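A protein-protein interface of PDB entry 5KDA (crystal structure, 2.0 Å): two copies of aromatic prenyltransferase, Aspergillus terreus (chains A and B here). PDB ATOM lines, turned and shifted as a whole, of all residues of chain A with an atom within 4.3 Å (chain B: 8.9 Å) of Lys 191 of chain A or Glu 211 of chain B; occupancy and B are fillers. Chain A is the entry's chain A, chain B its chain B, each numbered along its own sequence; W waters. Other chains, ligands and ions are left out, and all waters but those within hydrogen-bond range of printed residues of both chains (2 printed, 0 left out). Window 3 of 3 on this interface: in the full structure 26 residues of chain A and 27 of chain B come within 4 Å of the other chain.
Water W1 lies within hydrogen-bond range of the backbone carbonyl oxygen (O) of Ala 145 of chain A (2.6 Å) and the side-chain carboxylate (OE1) of Glu 211 of chain B (2.9 Å).
Water W2 lies within hydrogen-bond range of the side-chain amide oxygen (OE1) of Gln 146 of chain A, the backbone NH (N) of Glu 211 of chain B and a ring nitrogen (ND1) of His 142 of chain B.
Gln 209 of chain A touches its own counterpart, Gln 209 of chain B.
2 positions are printed for both chains.
Of the 8 pairs that touch across the chains among the printed residues, 1 has its exchanged pair printed and touching as well.
NZ of Lys 191 of chain A is in salt-bridge range of OE2 of Glu 211 of chain B, at 2.8 Å.
N of Glu 211 of chain B sits close to NE2 of Gln 209 of chain A.
The side-chain amide nitrogen (NE2) of Gln 209 of chain A sits at hydrogen-bond distance from the backbone carbonyl oxygen (O) of Gln 209 of chain B.
CB of Ala 145 of chain A touches O of Arg 138 of chain B (3.4 Å).
Ala 145 of chain A touches His 142 of chain B.
Gln 146 of chain A touches Glu 211 of chain B (O to OE1, 3.98 Å).
Leu 149 of chain A touches Arg 138 of chain B (CA to NH1, 3.7 Å).
Gln 209 of chain A touches Met 210 of chain B.
Of the printed residues of chain B, Gln 146 of chain A touches Glu 211.
No residue of chain B comes within 4 Å of Pro 190 of chain A.
Lys 191 of chain A touches just one residue of chain B: Glu 211.
Of the printed residues of chain B, Gln 209 of chain A touches Gln 209, Met 210 and Glu 211.
Of the printed residues of chain A, Arg 138 of chain B touches Ala 145 and Leu 149.
Printed residues of chain A within 4 Å of His 142 of chain B: Ala 145.
Printed residues of chain A within 4 Å of Gln 209 of chain B: Gln 209.
Of the printed residues of chain A, Glu 211 of chain B touches Gln 146, Lys 191 and Gln 209.
The nearest residue of chain B that does not touch Lys 191 of chain A is Lys 215 of chain B (5.4 Å).
The nearest printed residue of chain A that does not touch Met 210 of chain B is Gln 146 of chain A (5.4 Å).
The side-chain amide nitrogen (NE2) of Gln 146 of chain A sits close to the side-chain amide nitrogen (NE2) of Gln 209 of chain A.
NZ of Lys 215 of chain B lies within salt-bridge range of OE2 of Glu 211 of chain B (3.2 Å).
The side-chain amide nitrogen (NE2) of Gln 209 of chain B lies close to the side-chain amide nitrogen (NE2) of Gln 146 of chain B (3.0 Å).
The backbone carbonyl oxygen (O) of Lys 191 of chain A is in hydrogen-bond range of the side-chain hydroxyl (OG1) of Thr 195 of chain A, 2.6 Å away.
O of Ala 206 of chain B sits at hydrogen-bond distance from NE2 of His 142 of chain B (2.9 Å).
The side-chain amino group (NZ) of Lys 191 of chain A is in hydrogen-bond range of the backbone carbonyl oxygen (O) of Gln 146 of chain A (2.7 Å).
Of the 14 printed residues of chain A, 5 touch a printed residue of chain B.
Of the 23 printed residues of chain B, 5 touch a printed residue of chain A.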
ATOM      1  N   ALA A 145      24.941 -27.076 -10.512  1.00  0.00           N
ATOM      2  CA  ALA A 145      25.866 -26.306 -11.312  1.00  0.00           C
ATOM      3  C   ALA A 145      25.692 -26.539 -12.777  1.00  0.00           C
ATOM      4  O   ALA A 145      25.787 -25.580 -13.536  1.00  0.00           O
ATOM      5  CB  ALA A 145      27.328 -26.626 -10.972  1.00  0.00           C
ATOM      6  N   GLN A 146      25.479 -27.811 -13.173  1.00  0.00           N
ATOM      7  CA  GLN A 146      25.532 -28.243 -14.564  1.00  0.00           C
ATOM      8  C   GLN A 146      24.212 -28.107 -15.293  1.00  0.00           C
ATOM      9  O   GLN A 146      24.217 -27.873 -16.494  1.00  0.00           O
ATOM     10  CB  GLN A 146      25.943 -29.726 -14.668  1.00  0.00           C
ATOM     11  CG  GLN A 146      27.240 -30.052 -13.956  1.00  0.00           C
ATOM     12  CD  GLN A 146      28.438 -29.323 -14.555  1.00  0.00           C
ATOM     13  OE1 GLN A 146      29.182 -28.584 -13.881  1.00  0.00           O
ATOM     14  NE2 GLN A 146      28.624 -29.543 -15.813  1.00  0.00           N
ATOM     15  N   VAL A 147      23.084 -28.245 -14.607  1.00  0.00           N
ATOM     16  CA  VAL A 147      21.805 -28.084 -15.277  1.00  0.00           C
ATOM     17  C   VAL A 147      20.897 -26.979 -14.747  1.00  0.00           C
ATOM     18  O   VAL A 147      19.897 -26.690 -15.388  1.00  0.00           O
ATOM     19  CB  VAL A 147      21.033 -29.402 -15.409  1.00  0.00           C
ATOM     20  CG1 VAL A 147      21.894 -30.434 -16.106  1.00  0.00           C
ATOM     21  CG2 VAL A 147      20.575 -29.926 -14.092  1.00  0.00           C
ATOM     22  N   LEU A 149      19.881 -22.969 -13.887  1.00  0.00           N
ATOM     23  CA  LEU A 149      19.843 -21.825 -14.794  1.00  0.00           C
ATOM     24  C   LEU A 149      19.786 -20.562 -13.995  1.00  0.00           C
ATOM     25  O   LEU A 149      19.228 -20.584 -12.912  1.00  0.00           O
ATOM     26  CB  LEU A 149      18.589 -21.820 -15.651  1.00  0.00           C
ATOM     27  CG  LEU A 149      18.308 -22.966 -16.582  1.00  0.00           C
ATOM     28  CD1 LEU A 149      16.934 -22.773 -17.194  1.00  0.00           C
ATOM     29  CD2 LEU A 149      19.389 -23.027 -17.636  1.00  0.00           C
ATOM     30  N   THR A 188      16.483 -32.109 -17.176  1.00  0.00           N
ATOM     31  CA  THR A 188      17.316 -31.591 -18.251  1.00  0.00           C
ATOM     32  C   THR A 188      16.582 -30.652 -19.302  1.00  0.00           C
ATOM     33  O   THR A 188      17.250 -29.928 -20.080  1.00  0.00           O
ATOM     34  CB  THR A 188      17.833 -32.800 -19.016  1.00  0.00           C
ATOM     35  OG1 THR A 188      16.725 -33.511 -19.511  1.00  0.00           O
ATOM     36  CG2 THR A 188      18.566 -33.726 -18.089  1.00  0.00           C
ATOM     37  N   ILE A 189      15.248 -30.678 -19.294  1.00  0.00           N
ATOM     38  CA  ILE A 189      14.388 -29.983 -20.286  1.00  0.00           C
ATOM     39  C   ILE A 189      14.614 -28.432 -20.252  1.00  0.00           C
ATOM     40  O   ILE A 189      14.931 -27.797 -21.313  1.00  0.00           O
ATOM     41  CB  ILE A 189      12.895 -30.381 -20.097  1.00  0.00           C
ATOM     42  CG1 ILE A 189      12.665 -31.905 -20.212  1.00  0.00           C
ATOM     43  CG2 ILE A 189      11.929 -29.682 -21.057  1.00  0.00           C
ATOM     44  CD1 ILE A 189      12.444 -32.403 -21.568  1.00  0.00           C
ATOM     45  N   PRO A 190      14.517 -27.803 -19.054  1.00  0.00           N
ATOM     46  CA  PRO A 190      14.740 -26.351 -19.156  1.00  0.00           C
ATOM     47  C   PRO A 190      16.085 -25.917 -19.759  1.00  0.00           C
ATOM     48  O   PRO A 190      16.075 -25.007 -20.597  1.00  0.00           O
ATOM     49  CB  PRO A 190      14.531 -25.844 -17.724  1.00  0.00           C
ATOM     50  CG  PRO A 190      13.716 -26.894 -17.043  1.00  0.00           C
ATOM     51  CD  PRO A 190      14.216 -28.209 -17.658  1.00  0.00           C
ATOM     52  N   LYS A 191      17.224 -26.496 -19.328  1.00  0.00           N
ATOM     53  CA  LYS A 191      18.493 -26.204 -19.953  1.00  0.00           C
ATOM     54  C   LYS A 191      18.450 -26.532 -21.480  1.00  0.00           C
ATOM     55  O   LYS A 191      18.947 -25.776 -22.289  1.00  0.00           O
ATOM     56  CB  LYS A 191      19.677 -26.915 -19.268  1.00  0.00           C
ATOM     57  CG  LYS A 191      20.980 -26.671 -20.017  1.00  0.00           C
ATOM     58  CD  LYS A 191      22.213 -26.806 -19.124  1.00  0.00           C
ATOM     59  CE  LYS A 191      23.521 -26.810 -19.880  1.00  0.00           C
ATOM     60  NZ  LYS A 191      24.709 -26.878 -18.966  1.00  0.00           N
ATOM     61  N   GLY A 192      17.827 -27.637 -21.846  1.00  0.00           N
ATOM     62  CA  GLY A 192      17.709 -28.009 -23.243  1.00  0.00           C
ATOM     63  C   GLY A 192      17.042 -26.958 -24.112  1.00  0.00           C
ATOM     64  O   GLY A 192      17.568 -26.607 -25.161  1.00  0.00           O
ATOM     65  N   LEU A 193      15.893 -26.489 -23.635  1.00  0.00           N
ATOM     66  CA  LEU A 193      15.077 -25.519 -24.302  1.00  0.00           C
ATOM     67  C   LEU A 193      15.775 -24.215 -24.383  1.00  0.00           C
ATOM     68  O   LEU A 193      15.836 -23.613 -25.432  1.00  0.00           O
ATOM     69  CB  LEU A 193      13.765 -25.373 -23.582  1.00  0.00           C
ATOM     70  CG  LEU A 193      12.738 -26.486 -23.725  1.00  0.00           C
ATOM     71  CD1 LEU A 193      11.565 -26.133 -22.814  1.00  0.00           C
ATOM     72  CD2 LEU A 193      12.271 -26.679 -25.164  1.00  0.00           C
ATOM     73  N   VAL A 194      16.400 -23.802 -23.299  1.00  0.00           N
ATOM     74  CA  VAL A 194      16.999 -22.493 -23.235  1.00  0.00           C
ATOM     75  C   VAL A 194      18.298 -22.482 -24.046  1.00  0.00           C
ATOM     76  O   VAL A 194      18.519 -21.537 -24.776  1.00  0.00           O
ATOM     77  CB  VAL A 194      17.148 -22.018 -21.757  1.00  0.00           C
ATOM     78  CG1 VAL A 194      18.080 -20.842 -21.625  1.00  0.00           C
ATOM     79  CG2 VAL A 194      15.767 -21.682 -21.199  1.00  0.00           C
ATOM     80  N   THR A 195      19.106 -23.546 -23.984  1.00  0.00           N
ATOM     81  CA  THR A 195      20.381 -23.558 -24.681  1.00  0.00           C
ATOM     82  C   THR A 195      20.281 -24.087 -26.116  1.00  0.00           C
ATOM     83  O   THR A 195      21.264 -24.009 -26.839  1.00  0.00           O
ATOM     84  CB  THR A 195      21.386 -24.401 -23.938  1.00  0.00           C
ATOM     85  OG1 THR A 195      20.946 -25.789 -23.937  1.00  0.00           O
ATOM     86  CG2 THR A 195      21.524 -23.861 -22.537  1.00  0.00           C
ATOM     87  N   LEU A 202      23.561 -32.760 -23.222  1.00  0.00           N
ATOM     88  CA  LEU A 202      23.747 -31.997 -21.971  1.00  0.00           C
ATOM     89  C   LEU A 202      23.655 -32.903 -20.769  1.00  0.00           C
ATOM     90  O   LEU A 202      24.342 -32.643 -19.793  1.00  0.00           O
ATOM     91  CB  LEU A 202      22.804 -30.832 -21.887  1.00  0.00           C
ATOM     92  CG  LEU A 202      21.375 -31.171 -21.551  1.00  0.00           C
ATOM     93  CD1 LEU A 202      21.169 -31.068 -20.041  1.00  0.00           C
ATOM     94  CD2 LEU A 202      20.441 -30.202 -22.280  1.00  0.00           C
ATOM     95  N   GLN A 209      31.447 -34.692 -16.118  1.00  0.00           N
ATOM     96  CA  GLN A 209      32.215 -33.774 -15.311  1.00  0.00           C
ATOM     97  C   GLN A 209      32.229 -34.086 -13.805  1.00  0.00           C
ATOM     98  O   GLN A 209      32.918 -33.392 -13.062  1.00  0.00           O
ATOM     99  CB  GLN A 209      31.708 -32.343 -15.525  1.00  0.00           C
ATOM    100  CG  GLN A 209      32.091 -31.739 -16.862  1.00  0.00           C
ATOM    101  CD  GLN A 209      31.201 -30.548 -17.234  1.00  0.00           C
ATOM    102  OE1 GLN A 209      30.555 -30.512 -18.305  1.00  0.00           O
ATOM    103  NE2 GLN A 209      31.174 -29.544 -16.353  1.00  0.00           N
ATOM    104  N   ARG B 138      26.226 -20.714 -10.114  1.00  0.00           N
ATOM    105  CA  ARG B 138      26.654 -21.975 -10.710  1.00  0.00           C
ATOM    106  C   ARG B 138      28.109 -22.274 -10.449  1.00  0.00           C
ATOM    107  O   ARG B 138      28.442 -23.459 -10.214  1.00  0.00           O
ATOM    108  CB  ARG B 138      26.284 -22.025 -12.164  1.00  0.00           C
ATOM    109  CG  ARG B 138      24.779 -22.292 -12.331  1.00  0.00           C
ATOM    110  CD  ARG B 138      24.262 -22.130 -13.746  1.00  0.00           C
ATOM    111  NE  ARG B 138      24.459 -20.800 -14.316  1.00  0.00           N
ATOM    112  CZ  ARG B 138      23.966 -20.409 -15.481  1.00  0.00           C
ATOM    113  NH1 ARG B 138      23.262 -21.257 -16.219  1.00  0.00           N
ATOM    114  NH2 ARG B 138      24.172 -19.181 -15.916  1.00  0.00           N
ATOM    115  N   LEU B 139      28.960 -21.230 -10.383  1.00  0.00           N
ATOM    116  CA  LEU B 139      30.352 -21.489 -10.068  1.00  0.00           C
ATOM    117  C   LEU B 139      30.527 -21.770  -8.588  1.00  0.00           C
ATOM    118  O   LEU B 139      31.373 -22.587  -8.245  1.00  0.00           O
ATOM    119  CB  LEU B 139      31.295 -20.391 -10.536  1.00  0.00           C
ATOM    120  CG  LEU B 139      31.435 -20.202 -12.052  1.00  0.00           C
ATOM    121  CD1 LEU B 139      32.459 -19.111 -12.362  1.00  0.00           C
ATOM    122  CD2 LEU B 139      31.837 -21.468 -12.792  1.00  0.00           C
ATOM    123  N   HIS B 142      29.542 -25.406  -8.325  1.00  0.00           N
ATOM    124  CA  HIS B 142      30.602 -26.205  -8.907  1.00  0.00           C
ATOM    125  C   HIS B 142      31.749 -26.401  -7.909  1.00  0.00           C
ATOM    126  O   HIS B 142      32.083 -27.518  -7.588  1.00  0.00           O
ATOM    127  CB  HIS B 142      31.129 -25.600 -10.230  1.00  0.00           C
ATOM    128  CG  HIS B 142      32.327 -26.357 -10.752  1.00  0.00           C
ATOM    129  ND1 HIS B 142      32.210 -27.594 -11.326  1.00  0.00           N
ATOM    130  CD2 HIS B 142      33.653 -26.164 -10.549  1.00  0.00           C
ATOM    131  CE1 HIS B 142      33.417 -28.077 -11.579  1.00  0.00           C
ATOM    132  NE2 HIS B 142      34.309 -27.236 -11.105  1.00  0.00           N
ATOM    133  N   PHE B 143      32.330 -25.318  -7.365  1.00  0.00           N
ATOM    134  CA  PHE B 143      33.491 -25.482  -6.485  1.00  0.00           C
ATOM    135  C   PHE B 143      33.138 -26.024  -5.087  1.00  0.00           C
ATOM    136  O   PHE B 143      33.934 -26.718  -4.508  1.00  0.00           O
ATOM    137  CB  PHE B 143      34.288 -24.194  -6.455  1.00  0.00           C
ATOM    138  CG  PHE B 143      35.153 -24.032  -7.683  1.00  0.00           C
ATOM    139  CD1 PHE B 143      36.302 -24.864  -7.842  1.00  0.00           C
ATOM    140  CD2 PHE B 143      34.830 -23.154  -8.653  1.00  0.00           C
ATOM    141  CE1 PHE B 143      37.089 -24.772  -8.956  1.00  0.00           C
ATOM    142  CE2 PHE B 143      35.617 -23.054  -9.820  1.00  0.00           C
ATOM    143  CZ  PHE B 143      36.750 -23.863  -9.954  1.00  0.00           C
ATOM    144  N   GLN B 146      33.351 -29.654  -5.497  1.00  0.00           N
ATOM    145  CA  GLN B 146      34.675 -30.209  -5.692  1.00  0.00           C
ATOM    146  C   GLN B 146      35.521 -30.054  -4.463  1.00  0.00           C
ATOM    147  O   GLN B 146      36.365 -30.893  -4.219  1.00  0.00           O
ATOM    148  CB  GLN B 146      35.382 -29.540  -6.866  1.00  0.00           C
ATOM    149  CG  GLN B 146      34.557 -29.364  -8.127  1.00  0.00           C
ATOM    150  CD  GLN B 146      34.114 -30.667  -8.744  1.00  0.00           C
ATOM    151  OE1 GLN B 146      32.958 -30.820  -9.248  1.00  0.00           O
ATOM    152  NE2 GLN B 146      35.045 -31.608  -8.755  1.00  0.00           N
ATOM    153  N   ALA B 206      39.584 -29.667  -9.712  1.00  0.00           N
ATOM    154  CA  ALA B 206      38.327 -28.898  -9.569  1.00  0.00           C
ATOM    155  C   ALA B 206      38.150 -27.965 -10.765  1.00  0.00           C
ATOM    156  O   ALA B 206      37.102 -27.907 -11.403  1.00  0.00           O
ATOM    157  CB  ALA B 206      38.348 -28.144  -8.273  1.00  0.00           C
ATOM    158  N   ILE B 207      39.197 -27.274 -11.145  1.00  0.00           N
ATOM    159  CA  ILE B 207      39.082 -26.348 -12.263  1.00  0.00           C
ATOM    160  C   ILE B 207      38.866 -27.009 -13.625  1.00  0.00           C
ATOM    161  O   ILE B 207      38.148 -26.461 -14.465  1.00  0.00           O
ATOM    162  CB  ILE B 207      40.346 -25.470 -12.357  1.00  0.00           C
ATOM    163  CG1 ILE B 207      40.339 -24.467 -11.196  1.00  0.00           C
ATOM    164  CG2 ILE B 207      40.466 -24.760 -13.734  1.00  0.00           C
ATOM    165  CD1 ILE B 207      41.713 -23.896 -10.894  1.00  0.00           C
ATOM    166  N   GLU B 208      39.532 -28.133 -13.876  1.00  0.00           N
ATOM    167  CA  GLU B 208      39.410 -28.812 -15.172  1.00  0.00           C
ATOM    168  C   GLU B 208      38.024 -29.413 -15.370  1.00  0.00           C
ATOM    169  O   GLU B 208      37.625 -29.682 -16.516  1.00  0.00           O
ATOM    170  CB  GLU B 208      40.560 -29.825 -15.368  1.00  0.00           C
ATOM    171  CG  GLU B 208      41.869 -29.101 -15.712  1.00  0.00           C
ATOM    172  CD  GLU B 208      43.172 -29.729 -15.231  1.00  0.00           C
ATOM    173  OE1 GLU B 208      44.219 -29.030 -15.323  1.00  0.00           O
ATOM    174  OE2 GLU B 208      43.172 -30.890 -14.767  1.00  0.00           O
ATOM    175  N   GLN B 209      37.250 -29.564 -14.283  1.00  0.00           N
ATOM    176  CA  GLN B 209      35.886 -30.083 -14.365  1.00  0.00           C
ATOM    177  C   GLN B 209      34.843 -28.993 -14.544  1.00  0.00           C
ATOM    178  O   GLN B 209      33.651 -29.300 -14.642  1.00  0.00           O
ATOM    179  CB  GLN B 209      35.592 -31.024 -13.151  1.00  0.00           C
ATOM    180  CG  GLN B 209      36.170 -32.453 -13.356  1.00  0.00           C
ATOM    181  CD  GLN B 209      36.999 -33.025 -12.197  1.00  0.00           C
ATOM    182  OE1 GLN B 209      38.135 -33.533 -12.397  1.00  0.00           O
ATOM    183  NE2 GLN B 209      36.427 -32.997 -10.984  1.00  0.00           N
ATOM    184  N   MET B 210      35.244 -27.729 -14.618  1.00  0.00           N
ATOM    185  CA  MET B 210      34.261 -26.677 -14.813  1.00  0.00           C
ATOM    186  C   MET B 210      33.669 -26.811 -16.214  1.00  0.00           C
ATOM    187  O   MET B 210      34.402 -27.113 -17.201  1.00  0.00           O
ATOM    188  CB  MET B 210      34.894 -25.306 -14.709  1.00  0.00           C
ATOM    189  CG  MET B 210      35.541 -24.916 -13.386  1.00  0.00           C
ATOM    190  SD  MET B 210      36.450 -23.369 -13.653  1.00  0.00           S
ATOM    191  CE  MET B 210      35.186 -22.120 -13.789  1.00  0.00           C
ATOM    192  N   GLU B 211      32.373 -26.540 -16.321  1.00  0.00           N
ATOM    193  CA  GLU B 211      31.721 -26.426 -17.638  1.00  0.00           C
ATOM    194  C   GLU B 211      32.447 -25.441 -18.562  1.00  0.00           C
ATOM    195  O   GLU B 211      32.723 -25.770 -19.721  1.00  0.00           O
ATOM    196  CB  GLU B 211      30.233 -26.076 -17.515  1.00  0.00           C
ATOM    197  CG  GLU B 211      29.412 -26.414 -18.765  1.00  0.00           C
ATOM    198  CD  GLU B 211      27.950 -26.053 -18.600  1.00  0.00           C
ATOM    199  OE1 GLU B 211      27.515 -25.863 -17.435  1.00  0.00           O
ATOM    200  OE2 GLU B 211      27.227 -25.950 -19.624  1.00  0.00           O
ATOM    201  N   VAL B 212      32.839 -24.288 -18.038  1.00  0.00           N
ATOM    202  CA  VAL B 212      33.433 -23.245 -18.879  1.00  0.00           C
ATOM    203  C   VAL B 212      34.792 -23.617 -19.469  1.00  0.00           C
ATOM    204  O   VAL B 212      35.147 -23.161 -20.573  1.00  0.00           O
ATOM    205  CB  VAL B 212      33.540 -21.888 -18.143  1.00  0.00           C
ATOM    206  CG1 VAL B 212      32.197 -21.531 -17.539  1.00  0.00           C
ATOM    207  CG2 VAL B 212      34.632 -21.906 -17.061  1.00  0.00           C
ATOM    208  N   TYR B 213      35.517 -24.441 -18.724  1.00  0.00           N
ATOM    209  CA  TYR B 213      36.814 -24.959 -19.101  1.00  0.00           C
ATOM    210  C   TYR B 213      36.677 -25.829 -20.336  1.00  0.00           C
ATOM    211  O   TYR B 213      37.461 -25.698 -21.277  1.00  0.00           O
ATOM    212  CB  TYR B 213      37.376 -25.834 -17.962  1.00  0.00           C
ATOM    213  CG  TYR B 213      38.727 -26.447 -18.232  1.00  0.00           C
ATOM    214  CD1 TYR B 213      38.852 -27.675 -18.903  1.00  0.00           C
ATOM    215  CD2 TYR B 213      39.899 -25.792 -17.830  1.00  0.00           C
ATOM    216  CE1 TYR B 213      40.114 -28.232 -19.161  1.00  0.00           C
ATOM    217  CE2 TYR B 213      41.144 -26.327 -18.086  1.00  0.00           C
ATOM    218  CZ  TYR B 213      41.249 -27.538 -18.749  1.00  0.00           C
ATOM    219  OH  TYR B 213      42.486 -28.034 -18.985  1.00  0.00           O
ATOM    220  N   HIS B 214      35.720 -26.758 -20.285  1.00  0.00           N
ATOM    221  CA  HIS B 214      35.408 -27.614 -21.437  1.00  0.00           C
ATOM    222  C   HIS B 214      34.986 -26.771 -22.692  1.00  0.00           C
ATOM    223  O   HIS B 214      35.374 -27.071 -23.808  1.00  0.00           O
ATOM    224  CB  HIS B 214      34.389 -28.720 -21.038  1.00  0.00           C
ATOM    225  CG  HIS B 214      35.024 -29.919 -20.391  1.00  0.00           C
ATOM    226  ND1 HIS B 214      35.696 -30.886 -21.112  1.00  0.00           N
ATOM    227  CD2 HIS B 214      35.113 -30.296 -19.091  1.00  0.00           C
ATOM    228  CE1 HIS B 214      36.174 -31.803 -20.288  1.00  0.00           C
ATOM    229  NE2 HIS B 214      35.830 -31.472 -19.056  1.00  0.00           N
ATOM    230  N   LYS B 215      34.247 -25.694 -22.480  1.00  0.00           N
ATOM    231  CA  LYS B 215      33.770 -24.797 -23.558  1.00  0.00           C
ATOM    232  C   LYS B 215      34.802 -23.820 -24.197  1.00  0.00           C
ATOM    233  O   LYS B 215      34.534 -23.278 -25.267  1.00  0.00           O
ATOM    234  CB  LYS B 215      32.612 -23.913 -23.023  1.00  0.00           C
ATOM    235  CG  LYS B 215      31.211 -24.459 -23.211  1.00  0.00           C
ATOM    236  CD  LYS B 215      30.162 -23.357 -23.007  1.00  0.00           C
ATOM    237  CE  LYS B 215      28.749 -23.844 -23.341  1.00  0.00           C
ATOM    238  NZ  LYS B 215      28.305 -24.954 -22.440  1.00  0.00           N
ATOM    239  N   ASP B 216      35.931 -23.548 -23.533  1.00  0.00           N
ATOM    240  CA  ASP B 216      36.760 -22.347 -23.848  1.00  0.00           C
ATOM    241  C   ASP B 216      38.267 -22.635 -23.967  1.00  0.00           C
ATOM    242  O   ASP B 216      38.949 -22.797 -22.967  1.00  0.00           O
ATOM    243  CB  ASP B 216      36.531 -21.279 -22.783  1.00  0.00           C
ATOM    244  CG  ASP B 216      37.033 -19.936 -23.219  1.00  0.00           C
ATOM    245  OD1 ASP B 216      36.267 -19.275 -23.931  1.00  0.00           O
ATOM    246  OD2 ASP B 216      38.191 -19.546 -22.884  1.00  0.00           O
ATOM    247  N   ALA B 217      38.760 -22.709 -25.203  1.00  0.00           N
ATOM    248  CA  ALA B 217      40.161 -23.045 -25.502  1.00  0.00           C
ATOM    249  C   ALA B 217      41.235 -22.058 -24.966  1.00  0.00           C
ATOM    250  O   ALA B 217      42.281 -22.508 -24.470  1.00  0.00           O
ATOM    251  CB  ALA B 217      40.338 -23.247 -27.012  1.00  0.00           C
ATOM    252  N   LEU B 219      40.955 -20.089 -22.120  1.00  0.00           N
ATOM    253  CA  LEU B 219      41.080 -20.474 -20.716  1.00  0.00           C
ATOM    254  C   LEU B 219      41.945 -21.704 -20.514  1.00  0.00           C
ATOM    255  O   LEU B 219      42.791 -21.721 -19.636  1.00  0.00           O
ATOM    256  CB  LEU B 219      39.711 -20.738 -20.083  1.00  0.00           C
ATOM    257  CG  LEU B 219      39.612 -20.992 -18.569  1.00  0.00           C
ATOM    258  CD1 LEU B 219      40.308 -19.924 -17.726  1.00  0.00           C
ATOM    259  CD2 LEU B 219      38.127 -21.027 -18.187  1.00  0.00           C
ATOM    260  N   ARG B 220      41.744 -22.749 -21.315  1.00  0.00           N
ATOM    261  CA  ARG B 220      42.564 -23.970 -21.156  1.00  0.00           C
ATOM    262  C   ARG B 220      44.061 -23.693 -21.363  1.00  0.00           C
ATOM    263  O   ARG B 220      44.897 -24.238 -20.651  1.00  0.00           O
ATOM    264  CB  ARG B 220      42.094 -25.102 -22.078  1.00  0.00           C
ATOM    265  CG  ARG B 220      40.683 -25.598 -21.800  1.00  0.00           C
ATOM    266  CD  ARG B 220      40.385 -26.977 -22.407  1.00  0.00           C
ATOM    267  NE  ARG B 220      40.361 -26.873 -23.865  1.00  0.00           N
ATOM    268  CZ  ARG B 220      39.336 -26.440 -24.619  1.00  0.00           C
ATOM    269  NH1 ARG B 220      38.170 -26.090 -24.085  1.00  0.00           N
ATOM    270  NH2 ARG B 220      39.472 -26.366 -25.951  1.00  0.00           N
ATOM    271  N   ASP B 254      27.595 -14.827 -14.529  1.00  0.00           N
ATOM    272  CA  ASP B 254      27.565 -15.753 -15.661  1.00  0.00           C
ATOM    273  C   ASP B 254      28.925 -16.435 -15.776  1.00  0.00           C
ATOM    274  O   ASP B 254      29.922 -15.748 -15.861  1.00  0.00           O
ATOM    275  CB  ASP B 254      27.212 -14.938 -16.947  1.00  0.00           C
ATOM    276  CG  ASP B 254      27.118 -15.805 -18.223  1.00  0.00           C
ATOM    277  OD1 ASP B 254      27.118 -17.051 -18.155  1.00  0.00           O
ATOM    278  OD2 ASP B 254      27.041 -15.224 -19.320  1.00  0.00           O
ATOM    279  N   PRO B 255      29.008 -17.771 -15.701  1.00  0.00           N
ATOM    280  CA  PRO B 255      30.339 -18.378 -15.735  1.00  0.00           C
ATOM    281  C   PRO B 255      31.309 -17.903 -16.847  1.00  0.00           C
ATOM    282  O   PRO B 255      32.512 -17.813 -16.616  1.00  0.00           O
ATOM    283  CB  PRO B 255      30.026 -19.883 -15.845  1.00  0.00           C
ATOM    284  CG  PRO B 255      28.748 -20.047 -15.096  1.00  0.00           C
ATOM    285  CD  PRO B 255      27.979 -18.778 -15.369  1.00  0.00           C
ATOM    286  N   MET B 256      30.788 -17.566 -18.016  1.00  0.00           N
ATOM    287  CA  MET B 256      31.602 -17.036 -19.118  1.00  0.00           C
ATOM    288  C   MET B 256      32.271 -15.662 -18.867  1.00  0.00           C
ATOM    289  O   MET B 256      33.314 -15.385 -19.483  1.00  0.00           O
ATOM    290  CB  MET B 256      30.775 -17.001 -20.412  1.00  0.00           C
ATOM    291  CG  MET B 256      30.685 -18.375 -21.063  1.00  0.00           C
ATOM    292  SD  MET B 256      32.261 -18.745 -21.895  1.00  0.00           S
ATOM    293  CE  MET B 256      31.933 -20.433 -22.408  1.00  0.00           C
ATOM    294  N   PRO B 328      37.627 -16.521 -19.021  1.00  0.00           N
ATOM    295  CA  PRO B 328      37.232 -17.046 -20.345  1.00  0.00           C
ATOM    296  C   PRO B 328      37.492 -16.041 -21.495  1.00  0.00           C
ATOM    297  O   PRO B 328      37.278 -14.859 -21.323  1.00  0.00           O
ATOM    298  CB  PRO B 328      35.726 -17.304 -20.180  1.00  0.00           C
ATOM    299  CG  PRO B 328      35.565 -17.603 -18.724  1.00  0.00           C
ATOM    300  CD  PRO B 328      36.608 -16.790 -17.997  1.00  0.00           C
HETATM  301  O   HOH W   1      28.142 -25.136 -14.658  1.00  0.00           O
HETATM  302  O   HOH W   2      30.810 -26.224 -13.899  1.00  0.00           O
